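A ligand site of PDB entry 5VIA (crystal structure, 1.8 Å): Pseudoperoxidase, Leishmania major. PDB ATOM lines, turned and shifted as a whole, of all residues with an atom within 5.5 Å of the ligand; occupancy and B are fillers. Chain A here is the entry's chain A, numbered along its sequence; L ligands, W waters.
A ring nitrogen (NE2) of His 159 is bound to an iron atom (FE1) of the ligand (2.3 Å). FE1 of the ligand is bound by SG of Cys 60 (2.5 Å). N of Ser 169 lies close to O1 of the ligand (3.3 Å). The side-chain hydroxyl (OG) of Ser 169 lies within hydrogen-bond range of an oxygen (O1) of the ligand (2.5 Å). OG1 of Thr 36 is in hydrogen-bond range of O3 of the ligand (2.7 Å). The backbone NH (N) of His 165 is in hydrogen-bond range of an oxygen (O1) of the ligand, at 2.9 Å. ND1 of His 165 sits at hydrogen-bond distance from O2 of the ligand, 2.7 Å away. O4 of the ligand is in hydrogen-bond range of N of Glu 163, 3.0 Å away.
A ring nitrogen (ND1) of His 159 lies within hydrogen-bond range of the side-chain carboxylate of Glu 243, at 2.6 Å. The guanidinium group of Arg 39 lies within hydrogen-bond range of the backbone carbonyl oxygen of Cys 60 (2.7 Å). The side-chain hydroxyl of Thr 36 sits at hydrogen-bond distance from the backbone carbonyl oxygen of Asp 32, at 3.2 Å. The backbone NH of His 165 sits close to the backbone carbonyl oxygen of Leu 171, 3.2 Å away. The backbone carbonyl oxygen (O) of His 165 sits at hydrogen-bond distance from the backbone NH (N) of Gly 170 (3.2 Å). O of Val 56 lies within hydrogen-bond range of ND2 of Asn 240, 2.8 Å away. The side-chain amide nitrogen (ND2) of Asn 240 lies within hydrogen-bond range of the backbone carbonyl oxygen (O) of Asp 57 (3.3 Å). O of Leu 155 lies within hydrogen-bond range of SG of Cys 158.
Residues that only touch the ligand: Ala 35 (3.1 Å), Gly 162 (3.1 Å), Phe 164 (3.4 Å), Val 168 (3.4 Å), Asn 240 (3.4 Å), His 176 (3.4 Å), Glu 58 (3.4 Å), Phe 42 (3.5 Å), Ser 59 (3.5 Å), Cys 158 (3.5 Å), Arg 39 (3.6 Å), Met 277 (3.6 Å), Leu 141 (3.6 Å), Leu 155 (3.6 Å), Val 56 (3.6 Å), Ile 137 (3.7 Å), Ile 38 (3.8 Å), Leu 156 (3.9 Å) and Val 161 (3.99 Å). Hydrophobic or aromatic side chains within 4 Å of the ligand: Ala 35, Ile 38, Phe 42, Val 56, Ile 137, Leu 141, Leu 155, Leu 156, His 159, Phe 164, His 165, Val 168, His 176 and Met 277. Within 4 Å of the ligand: Ala 35, Thr 36, Ile 38, Arg 39, Phe 42, Val 56, Glu 58, Ser 59, Cys 60, Ile 137, Leu 141, Leu 155, Leu 156, Cys 158, His 159, Val 161, Gly 162, Glu 163, Phe 164, His 165, Val 168, Ser 169, His 176, Asn 240 and Met 277. The nearest printed residue that does not touch the ligand is Glu 243 (4.03 Å).
Water W1 lies within hydrogen-bond range of O3 of the ligand, NE of Arg 39 and ND1 of His 165. Water W2 bridges O4 of the ligand (2.6 Å) and O of Asp 32 (2.8 Å). Water W4 bridges the backbone carbonyl oxygen of Val 161 (2.6 Å) and a ring nitrogen (ND1) of His 176 (2.8 Å). Water W3 lies within hydrogen-bond range of OE2 of Glu 243, NE2 of His 176 and OD1 of Asn 240.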
ATOM      1  N   ASP A  32      -3.066  27.734   2.544  1.00  0.00           N
ATOM      2  CA  ASP A  32      -4.044  28.309   1.622  1.00  0.00           C
ATOM      3  C   ASP A  32      -4.787  27.252   0.836  1.00  0.00           C
ATOM      4  O   ASP A  32      -5.896  27.492   0.343  1.00  0.00           O
ATOM      5  CB  ASP A  32      -3.365  29.285   0.663  1.00  0.00           C
ATOM      6  CG  ASP A  32      -2.243  28.640  -0.156  1.00  0.00           C
ATOM      7  OD1 ASP A  32      -1.187  28.280   0.421  1.00  0.00           O
ATOM      8  OD2 ASP A  32      -2.416  28.510  -1.386  1.00  0.00           O
ATOM      9  N   ALA A  35      -8.617  25.602   2.013  1.00  0.00           N
ATOM     10  CA  ALA A  35      -9.879  26.114   1.492  1.00  0.00           C
ATOM     11  C   ALA A  35     -10.061  25.796  -0.009  1.00  0.00           C
ATOM     12  O   ALA A  35     -11.175  25.511  -0.459  1.00  0.00           O
ATOM     13  CB  ALA A  35     -10.018  27.589   1.762  1.00  0.00           C
ATOM     14  N   THR A  36      -8.969  25.843  -0.770  1.00  0.00           N
ATOM     15  CA  THR A  36      -9.086  25.497  -2.194  1.00  0.00           C
ATOM     16  C   THR A  36      -9.515  24.022  -2.374  1.00  0.00           C
ATOM     17  O   THR A  36     -10.282  23.698  -3.291  1.00  0.00           O
ATOM     18  CB  THR A  36      -7.803  25.785  -2.968  1.00  0.00           C
ATOM     19  OG1 THR A  36      -7.235  27.036  -2.534  1.00  0.00           O
ATOM     20  CG2 THR A  36      -8.105  25.847  -4.468  1.00  0.00           C
ATOM     21  N   ILE A  38     -11.440  22.457  -0.361  1.00  0.00           N
ATOM     22  CA  ILE A  38     -12.861  22.442  -0.039  1.00  0.00           C
ATOM     23  C   ILE A  38     -13.645  22.910  -1.253  1.00  0.00           C
ATOM     24  O   ILE A  38     -14.631  22.273  -1.635  1.00  0.00           O
ATOM     25  CB  ILE A  38     -13.198  23.347   1.170  1.00  0.00           C
ATOM     26  CG1 ILE A  38     -12.562  22.795   2.440  1.00  0.00           C
ATOM     27  CG2 ILE A  38     -14.728  23.490   1.328  1.00  0.00           C
ATOM     28  CD1 ILE A  38     -12.694  23.730   3.622  1.00  0.00           C
ATOM     29  N   ARG A  39     -13.191  24.002  -1.872  1.00  0.00           N
ATOM     30  CA  ARG A  39     -13.838  24.476  -3.082  1.00  0.00           C
ATOM     31  C   ARG A  39     -13.888  23.376  -4.141  1.00  0.00           C
ATOM     32  O   ARG A  39     -14.890  23.221  -4.834  1.00  0.00           O
ATOM     33  CB  ARG A  39     -13.135  25.708  -3.659  1.00  0.00           C
ATOM     34  CG  ARG A  39     -13.718  26.055  -5.033  1.00  0.00           C
ATOM     35  CD  ARG A  39     -13.391  27.465  -5.514  1.00  0.00           C
ATOM     36  NE  ARG A  39     -12.064  27.552  -6.060  1.00  0.00           N
ATOM     37  CZ  ARG A  39     -11.757  27.374  -7.338  1.00  0.00           C
ATOM     38  NH1 ARG A  39     -12.695  27.060  -8.221  1.00  0.00           N
ATOM     39  NH2 ARG A  39     -10.498  27.495  -7.719  1.00  0.00           N
ATOM     40  N   PHE A  42     -16.845  21.117  -4.278  1.00  0.00           N
ATOM     41  CA  PHE A  42     -17.948  21.755  -4.981  1.00  0.00           C
ATOM     42  C   PHE A  42     -17.747  21.791  -6.490  1.00  0.00           C
ATOM     43  O   PHE A  42     -18.669  21.481  -7.262  1.00  0.00           O
ATOM     44  CB  PHE A  42     -18.235  23.178  -4.438  1.00  0.00           C
ATOM     45  CG  PHE A  42     -19.192  23.974  -5.295  1.00  0.00           C
ATOM     46  CD1 PHE A  42     -20.480  23.488  -5.556  1.00  0.00           C
ATOM     47  CD2 PHE A  42     -18.820  25.193  -5.832  1.00  0.00           C
ATOM     48  CE1 PHE A  42     -21.370  24.219  -6.342  1.00  0.00           C
ATOM     49  CE2 PHE A  42     -19.695  25.923  -6.618  1.00  0.00           C
ATOM     50  CZ  PHE A  42     -20.970  25.435  -6.878  1.00  0.00           C
ATOM     51  N   VAL A  56     -17.264  33.326 -12.201  1.00  0.00           N
ATOM     52  CA  VAL A  56     -17.693  33.377 -10.792  1.00  0.00           C
ATOM     53  C   VAL A  56     -18.965  34.182 -10.593  1.00  0.00           C
ATOM     54  O   VAL A  56     -19.571  34.158  -9.514  1.00  0.00           O
ATOM     55  CB  VAL A  56     -16.576  33.907  -9.837  1.00  0.00           C
ATOM     56  CG1 VAL A  56     -15.350  33.008  -9.905  1.00  0.00           C
ATOM     57  CG2 VAL A  56     -16.210  35.359 -10.171  1.00  0.00           C
ATOM     58  N   ASP A  57     -19.387  34.900 -11.633  1.00  0.00           N
ATOM     59  CA  ASP A  57     -20.715  35.519 -11.616  1.00  0.00           C
ATOM     60  C   ASP A  57     -21.775  34.439 -11.383  1.00  0.00           C
ATOM     61  O   ASP A  57     -22.841  34.718 -10.821  1.00  0.00           O
ATOM     62  CB  ASP A  57     -20.983  36.282 -12.907  1.00  0.00           C
ATOM     63  CG  ASP A  57     -20.461  37.708 -12.869  1.00  0.00           C
ATOM     64  OD1 ASP A  57     -20.212  38.205 -11.740  1.00  0.00           O
ATOM     65  OD2 ASP A  57     -20.308  38.325 -13.946  1.00  0.00           O
ATOM     66  N   GLU A  58     -21.474  33.202 -11.787  1.00  0.00           N
ATOM     67  CA  GLU A  58     -22.391  32.071 -11.543  1.00  0.00           C
ATOM     68  C   GLU A  58     -22.077  31.332 -10.242  1.00  0.00           C
ATOM     69  O   GLU A  58     -22.915  31.249  -9.356  1.00  0.00           O
ATOM     70  CB  GLU A  58     -22.384  31.101 -12.725  1.00  0.00           C
ATOM     71  CG  GLU A  58     -23.423  29.970 -12.606  1.00  0.00           C
ATOM     72  CD  GLU A  58     -23.435  29.069 -13.828  1.00  0.00           C
ATOM     73  OE1 GLU A  58     -22.477  28.276 -13.990  1.00  0.00           O
ATOM     74  OE2 GLU A  58     -24.388  29.166 -14.641  1.00  0.00           O
ATOM     75  N   SER A  59     -20.862  30.782 -10.151  1.00  0.00           N
ATOM     76  CA  SER A  59     -20.382  30.151  -8.928  1.00  0.00           C
ATOM     77  C   SER A  59     -18.889  29.943  -9.060  1.00  0.00           C
ATOM     78  O   SER A  59     -18.319  30.226 -10.111  1.00  0.00           O
ATOM     79  CB  SER A  59     -21.053  28.785  -8.727  1.00  0.00           C
ATOM     80  OG  SER A  59     -20.451  27.812  -9.565  1.00  0.00           O
ATOM     81  N   CYS A  60     -18.259  29.432  -8.007  1.00  0.00           N
ATOM     82  CA  CYS A  60     -16.823  29.173  -8.084  1.00  0.00           C
ATOM     83  C   CYS A  60     -16.505  27.774  -8.629  1.00  0.00           C
ATOM     84  O   CYS A  60     -15.383  27.298  -8.490  1.00  0.00           O
ATOM     85  CB  CYS A  60     -16.158  29.367  -6.723  1.00  0.00           C
ATOM     86  SG  CYS A  60     -16.757  28.215  -5.476  1.00  0.00           S
ATOM     87  N   ILE A 137     -28.401  30.458  -7.910  1.00  0.00           N
ATOM     88  CA  ILE A 137     -27.755  29.718  -6.829  1.00  0.00           C
ATOM     89  C   ILE A 137     -28.587  28.517  -6.301  1.00  0.00           C
ATOM     90  O   ILE A 137     -28.048  27.421  -6.169  1.00  0.00           O
ATOM     91  CB  ILE A 137     -27.285  30.662  -5.696  1.00  0.00           C
ATOM     92  CG1 ILE A 137     -26.127  31.532  -6.212  1.00  0.00           C
ATOM     93  CG2 ILE A 137     -26.851  29.879  -4.466  1.00  0.00           C
ATOM     94  CD1 ILE A 137     -25.573  32.539  -5.185  1.00  0.00           C
ATOM     95  N   ILE A 140     -28.462  25.523  -8.736  1.00  0.00           N
ATOM     96  CA  ILE A 140     -27.216  24.788  -8.662  1.00  0.00           C
ATOM     97  C   ILE A 140     -27.131  23.967  -7.380  1.00  0.00           C
ATOM     98  O   ILE A 140     -26.858  22.773  -7.438  1.00  0.00           O
ATOM     99  CB  ILE A 140     -25.998  25.742  -8.763  1.00  0.00           C
ATOM    100  CG1 ILE A 140     -26.025  26.485 -10.104  1.00  0.00           C
ATOM    101  CG2 ILE A 140     -24.722  24.943  -8.599  1.00  0.00           C
ATOM    102  CD1 ILE A 140     -24.976  27.572 -10.227  1.00  0.00           C
ATOM    103  N   LEU A 141     -27.366  24.608  -6.237  1.00  0.00           N
ATOM    104  CA  LEU A 141     -27.128  23.947  -4.959  1.00  0.00           C
ATOM    105  C   LEU A 141     -28.093  22.782  -4.692  1.00  0.00           C
ATOM    106  O   LEU A 141     -27.680  21.746  -4.179  1.00  0.00           O
ATOM    107  CB  LEU A 141     -27.156  24.959  -3.812  1.00  0.00           C
ATOM    108  CG  LEU A 141     -26.082  26.067  -3.846  1.00  0.00           C
ATOM    109  CD1 LEU A 141     -26.130  26.902  -2.578  1.00  0.00           C
ATOM    110  CD2 LEU A 141     -24.686  25.479  -4.026  1.00  0.00           C
ATOM    111  N   LEU A 144     -27.047  19.376  -6.086  1.00  0.00           N
ATOM    112  CA  LEU A 144     -25.886  18.671  -5.535  1.00  0.00           C
ATOM    113  C   LEU A 144     -26.311  17.533  -4.607  1.00  0.00           C
ATOM    114  O   LEU A 144     -25.869  17.477  -3.465  1.00  0.00           O
ATOM    115  CB  LEU A 144     -24.986  19.656  -4.774  1.00  0.00           C
ATOM    116  CG  LEU A 144     -24.542  20.912  -5.545  1.00  0.00           C
ATOM    117  CD1 LEU A 144     -23.624  21.783  -4.699  1.00  0.00           C
ATOM    118  CD2 LEU A 144     -23.828  20.541  -6.824  1.00  0.00           C
ATOM    119  N   LEU A 155     -24.368  25.180   3.269  1.00  0.00           N
ATOM    120  CA  LEU A 155     -23.157  24.896   2.501  1.00  0.00           C
ATOM    121  C   LEU A 155     -22.379  26.169   2.225  1.00  0.00           C
ATOM    122  O   LEU A 155     -21.164  26.134   2.062  1.00  0.00           O
ATOM    123  CB  LEU A 155     -23.553  24.218   1.198  1.00  0.00           C
ATOM    124  CG  LEU A 155     -22.648  23.211   0.496  1.00  0.00           C
ATOM    125  CD1 LEU A 155     -21.870  22.278   1.464  1.00  0.00           C
ATOM    126  CD2 LEU A 155     -23.535  22.390  -0.445  1.00  0.00           C
ATOM    127  N   LEU A 156     -23.090  27.293   2.163  1.00  0.00           N
ATOM    128  CA  LEU A 156     -22.422  28.554   1.794  1.00  0.00           C
ATOM    129  C   LEU A 156     -21.487  29.112   2.859  1.00  0.00           C
ATOM    130  O   LEU A 156     -20.701  30.018   2.587  1.00  0.00           O
ATOM    131  CB  LEU A 156     -23.449  29.594   1.308  1.00  0.00           C
ATOM    132  CG  LEU A 156     -23.995  29.294  -0.108  1.00  0.00           C
ATOM    133  CD1 LEU A 156     -25.103  30.237  -0.464  1.00  0.00           C
ATOM    134  CD2 LEU A 156     -22.884  29.391  -1.157  1.00  0.00           C
ATOM    135  N   CYS A 158     -18.952  27.768   3.700  1.00  0.00           N
ATOM    136  CA  CYS A 158     -17.590  27.553   3.191  1.00  0.00           C
ATOM    137  C   CYS A 158     -16.976  28.877   2.751  1.00  0.00           C
ATOM    138  O   CYS A 158     -15.763  28.979   2.652  1.00  0.00           O
ATOM    139  CB  CYS A 158     -17.558  26.569   2.031  1.00  0.00           C
ATOM    140  SG  CYS A 158     -17.919  24.846   2.508  1.00  0.00           S
ATOM    141  N   HIS A 159     -17.812  29.871   2.489  1.00  0.00           N
ATOM    142  CA  HIS A 159     -17.294  31.210   2.145  1.00  0.00           C
ATOM    143  C   HIS A 159     -16.707  31.961   3.346  1.00  0.00           C
ATOM    144  O   HIS A 159     -16.189  33.072   3.200  1.00  0.00           O
ATOM    145  CB  HIS A 159     -18.408  32.043   1.509  1.00  0.00           C
ATOM    146  CG  HIS A 159     -18.660  31.690   0.071  1.00  0.00           C
ATOM    147  ND1 HIS A 159     -19.686  32.243  -0.659  1.00  0.00           N
ATOM    148  CD2 HIS A 159     -18.000  30.855  -0.761  1.00  0.00           C
ATOM    149  CE1 HIS A 159     -19.650  31.766  -1.890  1.00  0.00           C
ATOM    150  NE2 HIS A 159     -18.644  30.920  -1.972  1.00  0.00           N
ATOM    151  N   VAL A 161     -14.171  30.839   4.794  1.00  0.00           N
ATOM    152  CA  VAL A 161     -12.722  30.605   4.644  1.00  0.00           C
ATOM    153  C   VAL A 161     -12.276  30.888   3.215  1.00  0.00           C
ATOM    154  O   VAL A 161     -13.097  31.104   2.322  1.00  0.00           O
ATOM    155  CB  VAL A 161     -12.327  29.160   5.005  1.00  0.00           C
ATOM    156  CG1 VAL A 161     -12.600  28.854   6.473  1.00  0.00           C
ATOM    157  CG2 VAL A 161     -13.058  28.160   4.111  1.00  0.00           C
ATOM    158  N   GLY A 162     -10.963  30.870   2.993  1.00  0.00           N
ATOM    159  CA  GLY A 162     -10.405  31.051   1.672  1.00  0.00           C
ATOM    160  C   GLY A 162     -10.292  32.493   1.239  1.00  0.00           C
ATOM    161  O   GLY A 162     -10.542  33.403   2.027  1.00  0.00           O
ATOM    162  N   GLU A 163      -9.918  32.718  -0.014  1.00  0.00           N
ATOM    163  CA  GLU A 163      -9.817  34.071  -0.537  1.00  0.00           C
ATOM    164  C   GLU A 163      -9.965  34.099  -2.047  1.00  0.00           C
ATOM    165  O   GLU A 163     -10.100  33.057  -2.702  1.00  0.00           O
ATOM    166  CB  GLU A 163      -8.470  34.687  -0.148  1.00  0.00           C
ATOM    167  CG  GLU A 163      -7.278  33.816  -0.443  1.00  0.00           C
ATOM    168  CD  GLU A 163      -5.992  34.363   0.153  1.00  0.00           C
ATOM    169  OE1 GLU A 163      -5.522  35.416  -0.299  1.00  0.00           O
ATOM    170  OE2 GLU A 163      -5.461  33.742   1.085  1.00  0.00           O
ATOM    171  N   PHE A 164      -9.915  35.304  -2.604  1.00  0.00           N
ATOM    172  CA  PHE A 164     -10.045  35.525  -4.047  1.00  0.00           C
ATOM    173  C   PHE A 164      -8.711  35.412  -4.760  1.00  0.00           C
ATOM    174  O   PHE A 164      -7.677  35.789  -4.214  1.00  0.00           O
ATOM    175  CB  PHE A 164     -10.690  36.893  -4.287  1.00  0.00           C
ATOM    176  CG  PHE A 164     -12.169  36.914  -4.011  1.00  0.00           C
ATOM    177  CD1 PHE A 164     -12.665  36.701  -2.723  1.00  0.00           C
ATOM    178  CD2 PHE A 164     -13.071  37.109  -5.046  1.00  0.00           C
ATOM    179  CE1 PHE A 164     -14.031  36.706  -2.472  1.00  0.00           C
ATOM    180  CE2 PHE A 164     -14.453  37.101  -4.803  1.00  0.00           C
ATOM    181  CZ  PHE A 164     -14.925  36.907  -3.507  1.00  0.00           C
ATOM    182  N   HIS A 165      -8.727  34.905  -5.990  1.00  0.00           N
ATOM    183  CA  HIS A 165      -7.497  34.788  -6.777  1.00  0.00           C
ATOM    184  C   HIS A 165      -7.616  35.452  -8.152  1.00  0.00           C
ATOM    185  O   HIS A 165      -8.698  35.503  -8.762  1.00  0.00           O
ATOM    186  CB  HIS A 165      -7.115  33.304  -6.947  1.00  0.00           C
ATOM    187  CG  HIS A 165      -6.985  32.571  -5.654  1.00  0.00           C
ATOM    188  ND1 HIS A 165      -8.080  32.172  -4.910  1.00  0.00           N
ATOM    189  CD2 HIS A 165      -5.895  32.195  -4.943  1.00  0.00           C
ATOM    190  CE1 HIS A 165      -7.677  31.564  -3.814  1.00  0.00           C
ATOM    191  NE2 HIS A 165      -6.352  31.564  -3.805  1.00  0.00           N
ATOM    192  N   VAL A 168      -8.944  33.316 -11.047  1.00  0.00           N
ATOM    193  CA  VAL A 168     -10.279  32.761 -10.838  1.00  0.00           C
ATOM    194  C   VAL A 168     -11.332  33.864 -10.939  1.00  0.00           C
ATOM    195  O   VAL A 168     -12.112  33.910 -11.891  1.00  0.00           O
ATOM    196  CB  VAL A 168     -10.362  32.062  -9.476  1.00  0.00           C
ATOM    197  CG1 VAL A 168     -11.756  31.437  -9.250  1.00  0.00           C
ATOM    198  CG2 VAL A 168      -9.269  31.005  -9.369  1.00  0.00           C
ATOM    199  N   SER A 169     -11.350  34.769  -9.961  1.00  0.00           N
ATOM    200  CA  SER A 169     -12.298  35.890  -9.980  1.00  0.00           C
ATOM    201  C   SER A 169     -11.753  37.103 -10.701  1.00  0.00           C
ATOM    202  O   SER A 169     -12.511  37.951 -11.154  1.00  0.00           O
ATOM    203  CB  SER A 169     -12.697  36.276  -8.550  1.00  0.00           C
ATOM    204  OG  SER A 169     -13.296  35.175  -7.904  1.00  0.00           O
ATOM    205  N   GLY A 170     -10.427  37.209 -10.776  1.00  0.00           N
ATOM    206  CA  GLY A 170      -9.803  38.326 -11.443  1.00  0.00           C
ATOM    207  C   GLY A 170      -9.256  39.369 -10.480  1.00  0.00           C
ATOM    208  O   GLY A 170      -8.780  40.430 -10.914  1.00  0.00           O
ATOM    209  N   LEU A 171      -9.319  39.076  -9.187  1.00  0.00           N
ATOM    210  CA  LEU A 171      -8.776  39.983  -8.168  1.00  0.00           C
ATOM    211  C   LEU A 171      -8.148  39.189  -7.021  1.00  0.00           C
ATOM    212  O   LEU A 171      -8.448  38.016  -6.809  1.00  0.00           O
ATOM    213  CB  LEU A 171      -9.857  40.925  -7.647  1.00  0.00           C
ATOM    214  CG  LEU A 171     -11.012  40.142  -7.000  1.00  0.00           C
ATOM    215  CD1 LEU A 171     -11.219  40.529  -5.552  1.00  0.00           C
ATOM    216  CD2 LEU A 171     -12.305  40.335  -7.766  1.00  0.00           C
ATOM    217  N   HIS A 176     -14.433  36.760   1.388  1.00  0.00           N
ATOM    218  CA  HIS A 176     -15.858  37.009   1.517  1.00  0.00           C
ATOM    219  C   HIS A 176     -16.208  37.760   2.804  1.00  0.00           C
ATOM    220  O   HIS A 176     -17.102  38.621   2.818  1.00  0.00           O
ATOM    221  CB  HIS A 176     -16.653  35.702   1.484  1.00  0.00           C
ATOM    222  CG  HIS A 176     -16.815  35.110   0.118  1.00  0.00           C
ATOM    223  ND1 HIS A 176     -16.080  34.032  -0.329  1.00  0.00           N
ATOM    224  CD2 HIS A 176     -17.643  35.456  -0.901  1.00  0.00           C
ATOM    225  CE1 HIS A 176     -16.451  33.731  -1.566  1.00  0.00           C
ATOM    226  NE2 HIS A 176     -17.390  34.588  -1.936  1.00  0.00           N
ATOM    227  N   LEU A 219     -20.055  41.215  -8.813  1.00  0.00           N
ATOM    228  CA  LEU A 219     -19.408  41.220  -7.499  1.00  0.00           C
ATOM    229  C   LEU A 219     -19.735  42.499  -6.759  1.00  0.00           C
ATOM    230  O   LEU A 219     -19.839  43.573  -7.366  1.00  0.00           O
ATOM    231  CB  LEU A 219     -17.901  41.013  -7.610  1.00  0.00           C
ATOM    232  CG  LEU A 219     -17.399  39.699  -8.219  1.00  0.00           C
ATOM    233  CD1 LEU A 219     -15.882  39.655  -8.158  1.00  0.00           C
ATOM    234  CD2 LEU A 219     -18.000  38.474  -7.539  1.00  0.00           C
ATOM    235  N   ASN A 240     -20.834  37.841  -4.180  1.00  0.00           N
ATOM    236  CA  ASN A 240     -21.695  37.891  -5.367  1.00  0.00           C
ATOM    237  C   ASN A 240     -23.009  38.627  -5.070  1.00  0.00           C
ATOM    238  O   ASN A 240     -23.590  38.441  -4.001  1.00  0.00           O
ATOM    239  CB  ASN A 240     -22.040  36.467  -5.822  1.00  0.00           C
ATOM    240  CG  ASN A 240     -21.006  35.878  -6.741  1.00  0.00           C
ATOM    241  OD1 ASN A 240     -19.895  35.551  -6.318  1.00  0.00           O
ATOM    242  ND2 ASN A 240     -21.357  35.727  -8.026  1.00  0.00           N
ATOM    243  N   GLU A 243     -25.671  36.163  -4.024  1.00  0.00           N
ATOM    244  CA  GLU A 243     -25.622  35.702  -2.636  1.00  0.00           C
ATOM    245  C   GLU A 243     -26.318  36.702  -1.714  1.00  0.00           C
ATOM    246  O   GLU A 243     -26.946  36.312  -0.722  1.00  0.00           O
ATOM    247  CB  GLU A 243     -24.161  35.512  -2.216  1.00  0.00           C
ATOM    248  CG  GLU A 243     -23.769  34.083  -1.898  1.00  0.00           C
ATOM    249  CD  GLU A 243     -22.273  33.913  -1.712  1.00  0.00           C
ATOM    250  OE1 GLU A 243     -21.819  33.648  -0.564  1.00  0.00           O
ATOM    251  OE2 GLU A 243     -21.540  34.024  -2.716  1.00  0.00           O
ATOM    252  N   PHE A 274     -22.859  18.691   3.142  1.00  0.00           N
ATOM    253  CA  PHE A 274     -21.546  18.436   2.535  1.00  0.00           C
ATOM    254  C   PHE A 274     -21.442  16.979   2.141  1.00  0.00           C
ATOM    255  O   PHE A 274     -20.948  16.645   1.071  1.00  0.00           O
ATOM    256  CB  PHE A 274     -20.408  18.841   3.486  1.00  0.00           C
ATOM    257  CG  PHE A 274     -19.110  19.097   2.767  1.00  0.00           C
ATOM    258  CD1 PHE A 274     -18.266  18.050   2.461  1.00  0.00           C
ATOM    259  CD2 PHE A 274     -18.746  20.388   2.402  1.00  0.00           C
ATOM    260  CE1 PHE A 274     -17.053  18.273   1.793  1.00  0.00           C
ATOM    261  CE2 PHE A 274     -17.525  20.615   1.724  1.00  0.00           C
ATOM    262  CZ  PHE A 274     -16.690  19.549   1.430  1.00  0.00           C
ATOM    263  N   MET A 277     -23.413  16.417  -1.008  1.00  0.00           N
ATOM    264  CA  MET A 277     -22.667  16.972  -2.127  1.00  0.00           C
ATOM    265  C   MET A 277     -21.573  16.033  -2.608  1.00  0.00           C
ATOM    266  O   MET A 277     -21.448  15.785  -3.803  1.00  0.00           O
ATOM    267  CB  MET A 277     -22.054  18.325  -1.764  1.00  0.00           C
ATOM    268  CG  MET A 277     -21.325  18.962  -2.933  1.00  0.00           C
ATOM    269  SD  MET A 277     -20.569  20.541  -2.511  1.00  0.00           S
ATOM    270  CE  MET A 277     -19.306  19.994  -1.361  1.00  0.00           C
HETATM  271  C1  LIG L   1     -14.458  30.861  -3.303  1.00  0.00           C
HETATM  272  C2  LIG L   1     -18.605  32.399  -5.355  1.00  0.00           C
HETATM  273  C3  LIG L   1     -20.618  28.158  -4.069  1.00  0.00           C
HETATM  274  C4  LIG L   1     -16.710  26.985  -1.405  1.00  0.00           C
HETATM  275  C5  LIG L   1     -15.381  31.576  -4.018  1.00  0.00           C
HETATM  276  C6  LIG L   1     -15.086  32.779  -4.767  1.00  0.00           C
HETATM  277  C7  LIG L   1     -16.206  33.204  -5.344  1.00  0.00           C
HETATM  278  C8  LIG L   1     -17.284  32.286  -4.970  1.00  0.00           C
HETATM  279  C9  LIG L   1     -16.356  34.444  -6.235  1.00  0.00           C
HETATM  280  C10 LIG L   1     -13.690  33.406  -4.913  1.00  0.00           C
HETATM  281  C11 LIG L   1     -12.973  32.486  -5.924  1.00  0.00           C
HETATM  282  C12 LIG L   1     -11.556  32.913  -6.226  1.00  0.00           C
HETATM  283  O1  LIG L   1     -11.366  34.041  -6.749  1.00  0.00           O
HETATM  284  O2  LIG L   1     -10.613  32.106  -5.973  1.00  0.00           O
HETATM  285  C13 LIG L   1     -19.526  31.378  -5.215  1.00  0.00           C
HETATM  286  C14 LIG L   1     -20.899  31.372  -5.688  1.00  0.00           C
HETATM  287  C15 LIG L   1     -21.462  30.201  -5.355  1.00  0.00           C
HETATM  288  C16 LIG L   1     -20.475  29.424  -4.620  1.00  0.00           C
HETATM  289  C17 LIG L   1     -21.556  32.521  -6.466  1.00  0.00           C
HETATM  290  C18 LIG L   1     -22.931  29.841  -5.709  1.00  0.00           C
HETATM  291  C19 LIG L   1     -23.330  28.572  -5.872  1.00  0.00           C
HETATM  292  C20 LIG L   1     -19.754  27.479  -3.230  1.00  0.00           C
HETATM  293  C21 LIG L   1     -20.011  26.187  -2.579  1.00  0.00           C
HETATM  294  C22 LIG L   1     -18.910  25.862  -1.844  1.00  0.00           C
HETATM  295  C23 LIG L   1     -17.946  26.940  -2.009  1.00  0.00           C
HETATM  296  C24 LIG L   1     -21.328  25.369  -2.760  1.00  0.00           C
HETATM  297  C25 LIG L   1     -18.565  24.648  -0.959  1.00  0.00           C
HETATM  298  C26 LIG L   1     -19.321  23.543  -0.883  1.00  0.00           C
HETATM  299  C27 LIG L   1     -15.737  27.916  -1.643  1.00  0.00           C
HETATM  300  C28 LIG L   1     -14.426  27.948  -1.014  1.00  0.00           C
HETATM  301  C29 LIG L   1     -13.724  29.164  -1.609  1.00  0.00           C
HETATM  302  C30 LIG L   1     -14.681  29.744  -2.531  1.00  0.00           C
HETATM  303  C31 LIG L   1     -13.870  26.963   0.023  1.00  0.00           C
HETATM  304  C32 LIG L   1     -12.288  29.646  -1.302  1.00  0.00           C
HETATM  305  C33 LIG L   1     -11.391  28.887  -2.286  1.00  0.00           C
HETATM  306  C34 LIG L   1      -9.943  29.275  -2.149  1.00  0.00           C
HETATM  307  O3  LIG L   1      -9.124  28.881  -3.028  1.00  0.00           O
HETATM  308  O4  LIG L   1      -9.614  29.981  -1.163  1.00  0.00           O
HETATM  309  N1  LIG L   1     -16.744  31.306  -4.156  1.00  0.00           N
HETATM  310  N2  LIG L   1     -19.309  30.180  -4.568  1.00  0.00           N
HETATM  311  N3  LIG L   1     -18.477  27.907  -2.862  1.00  0.00           N
HETATM  312  N4  LIG L   1     -15.855  29.004  -2.515  1.00  0.00           N
HETATM  313 FE1  LIG L   1     -17.572  29.600  -3.587  1.00  0.00          FE
HETATM  314  O   HOH W   1      -9.796  29.341  -5.487  1.00  0.00           O
HETATM  315  O   HOH W   2      -7.118  29.887  -0.284  1.00  0.00           O
HETATM  316  O   HOH W   3     -19.465  35.225  -3.571  1.00  0.00           O
HETATM  317  O   HOH W   4     -14.457  31.882   0.233  1.00  0.00           O
